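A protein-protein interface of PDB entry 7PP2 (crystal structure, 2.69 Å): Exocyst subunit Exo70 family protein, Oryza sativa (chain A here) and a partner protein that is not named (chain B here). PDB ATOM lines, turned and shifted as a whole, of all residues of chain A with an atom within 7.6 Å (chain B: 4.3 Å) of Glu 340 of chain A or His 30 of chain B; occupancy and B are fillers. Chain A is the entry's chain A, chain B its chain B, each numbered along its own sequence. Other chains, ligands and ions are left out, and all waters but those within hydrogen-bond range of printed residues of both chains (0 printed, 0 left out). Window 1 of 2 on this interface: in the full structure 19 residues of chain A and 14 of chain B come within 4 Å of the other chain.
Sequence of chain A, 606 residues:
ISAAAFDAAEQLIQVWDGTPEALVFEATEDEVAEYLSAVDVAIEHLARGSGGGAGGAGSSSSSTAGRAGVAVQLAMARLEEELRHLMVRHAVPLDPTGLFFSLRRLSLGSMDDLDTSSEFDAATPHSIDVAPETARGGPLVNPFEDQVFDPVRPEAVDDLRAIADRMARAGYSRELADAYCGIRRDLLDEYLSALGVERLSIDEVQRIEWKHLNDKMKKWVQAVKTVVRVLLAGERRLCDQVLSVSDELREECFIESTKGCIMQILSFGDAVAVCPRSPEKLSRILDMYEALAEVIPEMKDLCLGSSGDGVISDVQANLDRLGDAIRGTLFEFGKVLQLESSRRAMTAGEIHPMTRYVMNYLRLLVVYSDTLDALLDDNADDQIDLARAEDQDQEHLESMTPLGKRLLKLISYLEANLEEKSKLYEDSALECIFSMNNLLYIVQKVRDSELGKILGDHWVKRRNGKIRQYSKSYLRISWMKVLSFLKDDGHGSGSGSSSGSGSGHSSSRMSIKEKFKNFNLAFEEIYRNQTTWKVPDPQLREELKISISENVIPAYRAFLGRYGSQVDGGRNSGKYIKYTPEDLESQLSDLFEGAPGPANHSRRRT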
ATOM      1  N   GLY A 334      28.540 -12.122  33.685  1.00  0.00           N
ATOM      2  CA  GLY A 334      27.172 -12.677  33.629  1.00  0.00           C
ATOM      3  C   GLY A 334      26.201 -11.860  34.466  1.00  0.00           C
ATOM      4  O   GLY A 334      25.042 -11.696  34.042  1.00  0.00           O
ATOM      5  N   LYS A 335      26.669 -11.358  35.611  1.00  0.00           N
ATOM      6  CA  LYS A 335      25.884 -10.544  36.576  1.00  0.00           C
ATOM      7  C   LYS A 335      25.510  -9.208  35.926  1.00  0.00           C
ATOM      8  O   LYS A 335      24.319  -8.853  35.949  1.00  0.00           O
ATOM      9  CB  LYS A 335      26.697 -10.350  37.860  1.00  0.00           C
ATOM     10  CG  LYS A 335      25.927  -9.787  39.045  1.00  0.00           C
ATOM     11  CD  LYS A 335      26.031  -8.285  39.177  1.00  0.00           C
ATOM     12  CE  LYS A 335      27.346  -7.829  39.769  1.00  0.00           C
ATOM     13  NZ  LYS A 335      27.504  -6.359  39.666  1.00  0.00           N
ATOM     14  N   VAL A 336      26.494  -8.512  35.350  1.00  0.00           N
ATOM     15  CA  VAL A 336      26.337  -7.164  34.724  1.00  0.00           C
ATOM     16  C   VAL A 336      25.488  -7.284  33.449  1.00  0.00           C
ATOM     17  O   VAL A 336      24.723  -6.346  33.169  1.00  0.00           O
ATOM     18  CB  VAL A 336      27.714  -6.523  34.457  1.00  0.00           C
ATOM     19  CG1 VAL A 336      27.640  -5.332  33.514  1.00  0.00           C
ATOM     20  CG2 VAL A 336      28.389  -6.120  35.759  1.00  0.00           C
ATOM     21  N   LEU A 337      25.617  -8.389  32.707  1.00  0.00           N
ATOM     22  CA  LEU A 337      24.796  -8.680  31.499  1.00  0.00           C
ATOM     23  C   LEU A 337      23.320  -8.796  31.898  1.00  0.00           C
ATOM     24  O   LEU A 337      22.478  -8.139  31.254  1.00  0.00           O
ATOM     25  CB  LEU A 337      25.289  -9.975  30.846  1.00  0.00           C
ATOM     26  CG  LEU A 337      24.535 -10.418  29.590  1.00  0.00           C
ATOM     27  CD1 LEU A 337      24.604  -9.359  28.498  1.00  0.00           C
ATOM     28  CD2 LEU A 337      25.076 -11.742  29.072  1.00  0.00           C
ATOM     29  N   GLN A 338      23.027  -9.602  32.924  1.00  0.00           N
ATOM     30  CA  GLN A 338      21.652  -9.854  33.441  1.00  0.00           C
ATOM     31  C   GLN A 338      21.031  -8.549  33.960  1.00  0.00           C
ATOM     32  O   GLN A 338      19.796  -8.411  33.868  1.00  0.00           O
ATOM     33  CB  GLN A 338      21.674 -10.910  34.547  1.00  0.00           C
ATOM     34  CG  GLN A 338      21.803 -12.333  34.026  1.00  0.00           C
ATOM     35  CD  GLN A 338      22.036 -13.327  35.136  1.00  0.00           C
ATOM     36  OE1 GLN A 338      21.109 -13.971  35.622  1.00  0.00           O
ATOM     37  NE2 GLN A 338      23.286 -13.455  35.552  1.00  0.00           N
ATOM     38  N   LEU A 339      21.850  -7.631  34.485  1.00  0.00           N
ATOM     39  CA  LEU A 339      21.380  -6.353  35.086  1.00  0.00           C
ATOM     40  C   LEU A 339      21.021  -5.334  33.992  1.00  0.00           C
ATOM     41  O   LEU A 339      20.288  -4.381  34.313  1.00  0.00           O
ATOM     42  CB  LEU A 339      22.458  -5.803  36.031  1.00  0.00           C
ATOM     43  CG  LEU A 339      22.578  -6.490  37.395  1.00  0.00           C
ATOM     44  CD1 LEU A 339      23.600  -5.777  38.272  1.00  0.00           C
ATOM     45  CD2 LEU A 339      21.236  -6.565  38.114  1.00  0.00           C
ATOM     46  N   GLU A 340      21.487  -5.518  32.751  1.00  0.00           N
ATOM     47  CA  GLU A 340      21.337  -4.508  31.665  1.00  0.00           C
ATOM     48  C   GLU A 340      19.880  -4.468  31.186  1.00  0.00           C
ATOM     49  O   GLU A 340      19.345  -5.538  30.828  1.00  0.00           O
ATOM     50  CB  GLU A 340      22.298  -4.797  30.512  1.00  0.00           C
ATOM     51  CG  GLU A 340      22.596  -3.563  29.685  1.00  0.00           C
ATOM     52  CD  GLU A 340      21.441  -3.093  28.821  1.00  0.00           C
ATOM     53  OE1 GLU A 340      20.871  -3.924  28.094  1.00  0.00           O
ATOM     54  OE2 GLU A 340      21.102  -1.900  28.897  1.00  0.00           O
ATOM     55  N   SER A 341      19.282  -3.271  31.157  1.00  0.00           N
ATOM     56  CA  SER A 341      17.815  -3.056  31.030  1.00  0.00           C
ATOM     57  C   SER A 341      17.471  -1.786  30.237  1.00  0.00           C
ATOM     58  O   SER A 341      16.331  -1.300  30.402  1.00  0.00           O
ATOM     59  CB  SER A 341      17.211  -3.002  32.402  1.00  0.00           C
ATOM     60  OG  SER A 341      17.828  -1.976  33.167  1.00  0.00           O
ATOM     61  N   SER A 342      18.382  -1.286  29.392  1.00  0.00           N
ATOM     62  CA  SER A 342      18.211  -0.032  28.608  1.00  0.00           C
ATOM     63  C   SER A 342      16.977  -0.142  27.707  1.00  0.00           C
ATOM     64  O   SER A 342      16.793  -1.194  27.064  1.00  0.00           O
ATOM     65  CB  SER A 342      19.433   0.312  27.790  1.00  0.00           C
ATOM     66  OG  SER A 342      19.131   1.303  26.813  1.00  0.00           O
ATOM     67  N   ARG A 343      16.178   0.925  27.667  1.00  0.00           N
ATOM     68  CA  ARG A 343      14.949   1.024  26.844  1.00  0.00           C
ATOM     69  C   ARG A 343      15.145   2.131  25.801  1.00  0.00           C
ATOM     70  O   ARG A 343      14.131   2.728  25.379  1.00  0.00           O
ATOM     71  CB  ARG A 343      13.744   1.234  27.765  1.00  0.00           C
ATOM     72  CG  ARG A 343      13.585   0.130  28.800  1.00  0.00           C
ATOM     73  CD  ARG A 343      12.244   0.145  29.511  1.00  0.00           C
ATOM     74  NE  ARG A 343      11.121   0.142  28.582  1.00  0.00           N
ATOM     75  CZ  ARG A 343      10.701  -0.911  27.878  1.00  0.00           C
ATOM     76  NH1 ARG A 343      11.310  -2.083  27.977  1.00  0.00           N
ATOM     77  NH2 ARG A 343       9.666  -0.783  27.066  1.00  0.00           N
ATOM     78  N   ARG A 344      16.398   2.384  25.399  1.00  0.00           N
ATOM     79  CA  ARG A 344      16.734   3.230  24.224  1.00  0.00           C
ATOM     80  C   ARG A 344      16.754   2.332  22.988  1.00  0.00           C
ATOM     81  O   ARG A 344      17.623   1.434  22.923  1.00  0.00           O
ATOM     82  CB  ARG A 344      18.082   3.943  24.373  1.00  0.00           C
ATOM     83  CG  ARG A 344      18.367   4.938  23.254  1.00  0.00           C
ATOM     84  CD  ARG A 344      19.738   5.586  23.320  1.00  0.00           C
ATOM     85  NE  ARG A 344      20.018   6.373  22.122  1.00  0.00           N
ATOM     86  CZ  ARG A 344      21.169   6.998  21.857  1.00  0.00           C
ATOM     87  NH1 ARG A 344      22.182   6.945  22.708  1.00  0.00           N
ATOM     88  NH2 ARG A 344      21.303   7.679  20.732  1.00  0.00           N
ATOM     89  N   HIS A 352      23.189  -3.865  18.008  1.00  0.00           N
ATOM     90  CA  HIS A 352      23.419  -3.225  19.332  1.00  0.00           C
ATOM     91  C   HIS A 352      24.885  -3.392  19.739  1.00  0.00           C
ATOM     92  O   HIS A 352      25.481  -4.446  19.513  1.00  0.00           O
ATOM     93  CB  HIS A 352      22.449  -3.795  20.376  1.00  0.00           C
ATOM     94  CG  HIS A 352      22.290  -2.928  21.578  1.00  0.00           C
ATOM     95  ND1 HIS A 352      21.192  -2.115  21.759  1.00  0.00           N
ATOM     96  CD2 HIS A 352      23.083  -2.737  22.651  1.00  0.00           C
ATOM     97  CE1 HIS A 352      21.319  -1.456  22.895  1.00  0.00           C
ATOM     98  NE2 HIS A 352      22.475  -1.822  23.460  1.00  0.00           N
ATOM     99  N   PRO A 353      25.525  -2.359  20.340  1.00  0.00           N
ATOM    100  CA  PRO A 353      26.928  -2.454  20.749  1.00  0.00           C
ATOM    101  C   PRO A 353      27.218  -3.602  21.729  1.00  0.00           C
ATOM    102  O   PRO A 353      28.276  -4.188  21.654  1.00  0.00           O
ATOM    103  CB  PRO A 353      27.185  -1.102  21.434  1.00  0.00           C
ATOM    104  CG  PRO A 353      26.189  -0.171  20.793  1.00  0.00           C
ATOM    105  CD  PRO A 353      24.956  -1.028  20.616  1.00  0.00           C
ATOM    106  N   MET A 354      26.291  -3.843  22.655  1.00  0.00           N
ATOM    107  CA  MET A 354      26.294  -4.981  23.609  1.00  0.00           C
ATOM    108  C   MET A 354      26.477  -6.293  22.846  1.00  0.00           C
ATOM    109  O   MET A 354      27.278  -7.119  23.304  1.00  0.00           O
ATOM    110  CB  MET A 354      24.979  -5.025  24.393  1.00  0.00           C
ATOM    111  CG  MET A 354      24.765  -6.302  25.174  1.00  0.00           C
ATOM    112  SD  MET A 354      23.576  -6.046  26.499  1.00  0.00           S
ATOM    113  CE  MET A 354      24.632  -5.159  27.638  1.00  0.00           C
ATOM    114  N   THR A 355      25.754  -6.476  21.738  1.00  0.00           N
ATOM    115  CA  THR A 355      25.835  -7.686  20.877  1.00  0.00           C
ATOM    116  C   THR A 355      27.278  -7.844  20.381  1.00  0.00           C
ATOM    117  O   THR A 355      27.796  -8.976  20.434  1.00  0.00           O
ATOM    118  CB  THR A 355      24.853  -7.621  19.700  1.00  0.00           C
ATOM    119  OG1 THR A 355      23.588  -7.161  20.174  1.00  0.00           O
ATOM    120  CG2 THR A 355      24.681  -8.956  19.007  1.00  0.00           C
ATOM    121  N   TYR A 357      30.072  -6.462  21.777  1.00  0.00           N
ATOM    122  CA  TYR A 357      30.959  -6.631  22.958  1.00  0.00           C
ATOM    123  C   TYR A 357      30.821  -8.051  23.516  1.00  0.00           C
ATOM    124  O   TYR A 357      31.863  -8.726  23.688  1.00  0.00           O
ATOM    125  CB  TYR A 357      30.661  -5.603  24.052  1.00  0.00           C
ATOM    126  CG  TYR A 357      31.575  -5.720  25.247  1.00  0.00           C
ATOM    127  CD1 TYR A 357      32.793  -5.064  25.276  1.00  0.00           C
ATOM    128  CD2 TYR A 357      31.243  -6.515  26.332  1.00  0.00           C
ATOM    129  CE1 TYR A 357      33.648  -5.176  26.360  1.00  0.00           C
ATOM    130  CE2 TYR A 357      32.088  -6.642  27.424  1.00  0.00           C
ATOM    131  CZ  TYR A 357      33.297  -5.970  27.439  1.00  0.00           C
ATOM    132  OH  TYR A 357      34.145  -6.078  28.506  1.00  0.00           O
ATOM    133  N   TYR A 413      20.956 -15.034  27.843  1.00  0.00           N
ATOM    134  CA  TYR A 413      20.763 -13.719  28.508  1.00  0.00           C
ATOM    135  C   TYR A 413      20.822 -12.609  27.458  1.00  0.00           C
ATOM    136  O   TYR A 413      19.956 -11.717  27.496  1.00  0.00           O
ATOM    137  CB  TYR A 413      21.813 -13.477  29.597  1.00  0.00           C
ATOM    138  CG  TYR A 413      21.771 -14.417  30.777  1.00  0.00           C
ATOM    139  CD1 TYR A 413      20.598 -15.047  31.169  1.00  0.00           C
ATOM    140  CD2 TYR A 413      22.910 -14.648  31.532  1.00  0.00           C
ATOM    141  CE1 TYR A 413      20.564 -15.897  32.262  1.00  0.00           C
ATOM    142  CE2 TYR A 413      22.893 -15.496  32.628  1.00  0.00           C
ATOM    143  CZ  TYR A 413      21.715 -16.123  32.993  1.00  0.00           C
ATOM    144  OH  TYR A 413      21.690 -16.961  34.066  1.00  0.00           O
ATOM    145  N   ASN A 417      17.664 -10.346  26.397  1.00  0.00           N
ATOM    146  CA  ASN A 417      17.824  -8.872  26.517  1.00  0.00           C
ATOM    147  C   ASN A 417      17.441  -8.224  25.181  1.00  0.00           C
ATOM    148  O   ASN A 417      16.658  -7.251  25.201  1.00  0.00           O
ATOM    149  CB  ASN A 417      19.243  -8.506  26.970  1.00  0.00           C
ATOM    150  CG  ASN A 417      19.505  -7.014  27.057  1.00  0.00           C
ATOM    151  OD1 ASN A 417      18.889  -6.219  26.351  1.00  0.00           O
ATOM    152  ND2 ASN A 417      20.438  -6.622  27.909  1.00  0.00           N
ATOM    153  N   LEU A 418      17.969  -8.744  24.069  1.00  0.00           N
ATOM    154  CA  LEU A 418      17.781  -8.173  22.704  1.00  0.00           C
ATOM    155  C   LEU A 418      16.314  -8.294  22.272  1.00  0.00           C
ATOM    156  O   LEU A 418      15.848  -7.392  21.546  1.00  0.00           O
ATOM    157  CB  LEU A 418      18.707  -8.885  21.711  1.00  0.00           C
ATOM    158  CG  LEU A 418      20.178  -8.487  21.787  1.00  0.00           C
ATOM    159  CD1 LEU A 418      21.041  -9.445  20.980  1.00  0.00           C
ATOM    160  CD2 LEU A 418      20.380  -7.060  21.308  1.00  0.00           C
ATOM    161  N   LYS A 421      14.465  -5.456  23.635  1.00  0.00           N
ATOM    162  CA  LYS A 421      14.933  -4.242  22.911  1.00  0.00           C
ATOM    163  C   LYS A 421      14.238  -4.146  21.547  1.00  0.00           C
ATOM    164  O   LYS A 421      14.112  -3.014  21.038  1.00  0.00           O
ATOM    165  CB  LYS A 421      16.455  -4.244  22.730  1.00  0.00           C
ATOM    166  CG  LYS A 421      17.265  -3.969  23.988  1.00  0.00           C
ATOM    167  CD  LYS A 421      18.609  -3.335  23.704  1.00  0.00           C
ATOM    168  CE  LYS A 421      19.585  -3.467  24.855  1.00  0.00           C
ATOM    169  NZ  LYS A 421      19.109  -2.766  26.070  1.00  0.00           N
ATOM    170  N   THR B  28      20.794   6.240  27.177  1.00  0.00           N
ATOM    171  CA  THR B  28      22.046   5.490  26.887  1.00  0.00           C
ATOM    172  C   THR B  28      21.698   4.040  26.523  1.00  0.00           C
ATOM    173  O   THR B  28      20.708   3.515  27.065  1.00  0.00           O
ATOM    174  CB  THR B  28      23.044   5.607  28.046  1.00  0.00           C
ATOM    175  OG1 THR B  28      22.505   4.969  29.205  1.00  0.00           O
ATOM    176  CG2 THR B  28      23.393   7.045  28.367  1.00  0.00           C
ATOM    177  N   TYR B  29      22.486   3.430  25.632  1.00  0.00           N
ATOM    178  CA  TYR B  29      22.248   2.081  25.047  1.00  0.00           C
ATOM    179  C   TYR B  29      22.417   0.995  26.113  1.00  0.00           C
ATOM    180  O   TYR B  29      21.874  -0.101  25.915  1.00  0.00           O
ATOM    181  CB  TYR B  29      23.195   1.817  23.872  1.00  0.00           C
ATOM    182  CG  TYR B  29      22.920   2.638  22.635  1.00  0.00           C
ATOM    183  CD1 TYR B  29      21.669   2.635  22.038  1.00  0.00           C
ATOM    184  CD2 TYR B  29      23.914   3.405  22.046  1.00  0.00           C
ATOM    185  CE1 TYR B  29      21.409   3.382  20.901  1.00  0.00           C
ATOM    186  CE2 TYR B  29      23.672   4.153  20.905  1.00  0.00           C
ATOM    187  CZ  TYR B  29      22.415   4.141  20.331  1.00  0.00           C
ATOM    188  OH  TYR B  29      22.163   4.873  19.209  1.00  0.00           O
ATOM    189  N   HIS B  30      23.180   1.290  27.172  1.00  0.00           N
ATOM    190  CA  HIS B  30      23.393   0.431  28.370  1.00  0.00           C
ATOM    191  C   HIS B  30      22.816   1.142  29.597  1.00  0.00           C
ATOM    192  O   HIS B  30      23.055   2.354  29.724  1.00  0.00           O
ATOM    193  CB  HIS B  30      24.883   0.118  28.565  1.00  0.00           C
ATOM    194  CG  HIS B  30      25.591  -0.270  27.310  1.00  0.00           C
ATOM    195  ND1 HIS B  30      26.235   0.652  26.502  1.00  0.00           N
ATOM    196  CD2 HIS B  30      25.759  -1.473  26.719  1.00  0.00           C
ATOM    197  CE1 HIS B  30      26.765   0.031  25.468  1.00  0.00           C
ATOM    198  NE2 HIS B  30      26.490  -1.276  25.581  1.00  0.00           N
ATOM    199  N   LYS B  31      22.077   0.417  30.445  1.00  0.00           N
ATOM    200  CA  LYS B  31      21.483   0.934  31.712  1.00  0.00           C
ATOM    201  C   LYS B  31      21.403  -0.186  32.753  1.00  0.00           C
ATOM    202  O   LYS B  31      20.746  -1.210  32.475  1.00  0.00           O
ATOM    203  CB  LYS B  31      20.087   1.514  31.472  1.00  0.00           C
ATOM    204  CG  LYS B  31      19.966   3.004  31.748  1.00  0.00           C
ATOM    205  CD  LYS B  31      20.010   3.348  33.217  1.00  0.00           C
ATOM    206  CE  LYS B  31      19.601   4.780  33.488  1.00  0.00           C
ATOM    207  NZ  LYS B  31      20.472   5.741  32.770  1.00  0.00           N
ATOM    208  N   GLY B  38      24.485   4.315  33.333  1.00  0.00           N
ATOM    209  CA  GLY B  38      24.212   4.211  31.888  1.00  0.00           C
ATOM    210  C   GLY B  38      25.362   4.759  31.056  1.00  0.00           C
ATOM    211  O   GLY B  38      26.074   5.665  31.534  1.00  0.00           O
ATOM    212  N   SER B  39      25.538   4.224  29.848  1.00  0.00           N
ATOM    213  CA  SER B  39      26.616   4.596  28.895  1.00  0.00           C
ATOM    214  C   SER B  39      26.293   4.000  27.528  1.00  0.00           C
ATOM    215  O   SER B  39      25.637   2.948  27.497  1.00  0.00           O
ATOM    216  CB  SER B  39      27.964   4.132  29.385  1.00  0.00           C
ATOM    217  OG  SER B  39      28.930   4.198  28.345  1.00  0.00           O
ATOM    218  N   ASP B  40      26.735   4.655  26.452  1.00  0.00           N
ATOM    219  CA  ASP B  40      26.583   4.164  25.056  1.00  0.00           C
ATOM    220  C   ASP B  40      27.765   3.249  24.706  1.00  0.00           C
ATOM    221  O   ASP B  40      27.733   2.657  23.619  1.00  0.00           O
ATOM    222  CB  ASP B  40      26.420   5.337  24.086  1.00  0.00           C
ATOM    223  CG  ASP B  40      25.080   6.046  24.224  1.00  0.00           C
ATOM    224  OD1 ASP B  40      24.079   5.356  24.486  1.00  0.00           O
ATOM    225  OD2 ASP B  40      25.047   7.281  24.068  1.00  0.00           O
ATOM    226  N   ASP B  41      28.745   3.126  25.607  1.00  0.00           N
ATOM    227  CA  ASP B  41      29.986   2.320  25.445  1.00  0.00           C
ATOM    228  C   ASP B  41      29.850   1.051  26.289  1.00  0.00           C
ATOM    229  O   ASP B  41      29.640   1.173  27.511  1.00  0.00           O
ATOM    230  CB  ASP B  41      31.218   3.132  25.861  1.00  0.00           C
ATOM    231  CG  ASP B  41      32.558   2.488  25.543  1.00  0.00           C
ATOM    232  OD1 ASP B  41      32.870   2.336  24.345  1.00  0.00           O
ATOM    233  OD2 ASP B  41      33.293   2.163  26.502  1.00  0.00           O
ATOM    234  N   SER B  42      29.969  -0.119  25.659  1.00  0.00           N
ATOM    235  CA  SER B  42      29.796  -1.449  26.296  1.00  0.00           C
ATOM    236  C   SER B  42      30.920  -1.690  27.310  1.00  0.00           C
ATOM    237  O   SER B  42      30.612  -2.109  28.444  1.00  0.00           O
ATOM    238  CB  SER B  42      29.738  -2.535  25.262  1.00  0.00           C
ATOM    239  OG  SER B  42      28.652  -2.316  24.377  1.00  0.00           O
ATOM    240  N   TYR B  45      30.302   0.160  30.386  1.00  0.00           N
ATOM    241  CA  TYR B  45      29.137  -0.449  31.077  1.00  0.00           C
ATOM    242  C   TYR B  45      29.568  -1.738  31.786  1.00  0.00           C
ATOM    243  O   TYR B  45      29.241  -1.898  32.972  1.00  0.00           O
ATOM    244  CB  TYR B  45      27.966  -0.746  30.138  1.00  0.00           C
ATOM    245  CG  TYR B  45      26.888  -1.524  30.850  1.00  0.00           C
ATOM    246  CD1 TYR B  45      26.079  -0.910  31.790  1.00  0.00           C
ATOM    247  CD2 TYR B  45      26.744  -2.891  30.668  1.00  0.00           C
ATOM    248  CE1 TYR B  45      25.121  -1.619  32.495  1.00  0.00           C
ATOM    249  CE2 TYR B  45      25.793  -3.616  31.367  1.00  0.00           C
ATOM    250  CZ  TYR B  45      24.980  -2.978  32.286  1.00  0.00           C
ATOM    251  OH  TYR B  45      24.038  -3.677  32.981  1.00  0.00           O
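The guanidinium group (NH1) of Arg 344 of chain A lies within salt-bridge range of the side-chain carboxylate (OD1) of Asp 40 of chain B (3.0 Å).
N of Ser 341 of chain A is in hydrogen-bond range of O of Lys 31 of chain B, 2.9 Å away.
The side-chain hydroxyl of Ser 42 of chain B lies close to the backbone carbonyl oxygen of Pro 353 of chain A, at 3.3 Å.
NH2 of Arg 344 of chain A lies within hydrogen-bond range of OH of Tyr 29 of chain B, at 3.3 Å.
The side-chain hydroxyl (OG) of Ser 42 of chain B lies within hydrogen-bond range of the backbone NH (N) of Met 354 of chain A (3.3 Å).
OE2 of Glu 340 of chain A is in hydrogen-bond range of N of Lys 31 of chain B (3.0 Å).
A ring nitrogen (NE2) of His 352 of chain A is in hydrogen-bond range of the backbone carbonyl oxygen of Tyr 29 of chain B.
The backbone carbonyl oxygen (O) of Val 336 of chain A is in hydrogen-bond range of the side-chain hydroxyl (OH) of Tyr 45 of chain B, 2.8 Å away.
OG of Ser 342 of chain A sits at hydrogen-bond distance from O of Thr 28 of chain B (2.7 Å).
The backbone NH of Glu 340 of chain A sits close to the side-chain hydroxyl of Tyr 45 of chain B, 3.2 Å away.
The side-chain hydroxyl of Ser 342 of chain A sits close to the backbone carbonyl oxygen of Tyr 29 of chain B, 3.2 Å away.
The side-chain hydroxyl (OG) of Ser 42 of chain B is in hydrogen-bond range of a ring nitrogen (NE2) of His 30 of chain B, 2.7 Å away.
The side-chain hydroxyl of Thr 355 of chain A sits close to the backbone carbonyl oxygen of His 352 of chain A (3.4 Å).
The backbone NH (N) of Ser 342 of chain A is in hydrogen-bond range of the side-chain carboxylate (OE2) of Glu 340 of chain A (2.8 Å).
The side-chain amide oxygen of Asn 417 of chain A lies close to the side-chain amino group of Lys 421 of chain A.
OG1 of Thr 28 of chain B is in hydrogen-bond range of O of His 30 of chain B.
The side-chain amino group (NZ) of Lys 421 of chain A sits at hydrogen-bond distance from the backbone carbonyl oxygen (O) of Ser 342 of chain A (3.0 Å).
O of Leu 339 of chain A touches O of Lys 31 of chain B, at 3.7 Å.
Leu 339 of chain A touches Tyr 45 of chain B.
Glu 340 of chain A touches Tyr 29 of chain B (OE2 to O, 3.6 Å).
CA of His 30 of chain B touches OE2 of Glu 340 of chain A, at 3.3 Å.
CB of Ser 342 of chain A touches N of His 30 of chain B, 3.9 Å away.
Ser 342 of chain A touches Lys 31 of chain B (CB to N, 3.7 Å).
CB of Arg 344 of chain A touches O of Thr 28 of chain B, 3.8 Å away.
N of Met 354 of chain A touches NE2 of His 30 of chain B (3.9 Å).
Ser 42 of chain B touches Tyr 357 of chain A.
NZ of Lys 421 of chain A touches O of Tyr 29 of chain B, at 3.8 Å.
Printed residues of chain B within 4 Å of Val 336 of chain A: Tyr 45 (2.8 Å).
Glu 340 of chain A touches four residues of chain B.
Arg 343 of chain A touches none of the printed residues of chain B.
Of the printed residues of chain B, Pro 353 of chain A touches Ser 42.
Of the printed residues of chain B, Tyr 357 of chain A touches Ser 42.
His 30 of chain B touches just these residues of chain A: Glu 340, Ser 342 and Met 354.
Of the 20 printed residues of chain A, 11 touch a printed residue of chain B.
Hydrophobic or aromatic side chains of chain A that line the printed part of chain B: Val 336, His 352, Pro 353, Met 354 and Tyr 357.
Of the 10 printed residues of chain B, 7 touch a printed residue of chain A.
Among the printed residues, Asp or Glu carboxylates within 4 Å of a Lys or Arg side-chain nitrogen of the other chain: Arg 344 of chain A with Asp 40 of chain B.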
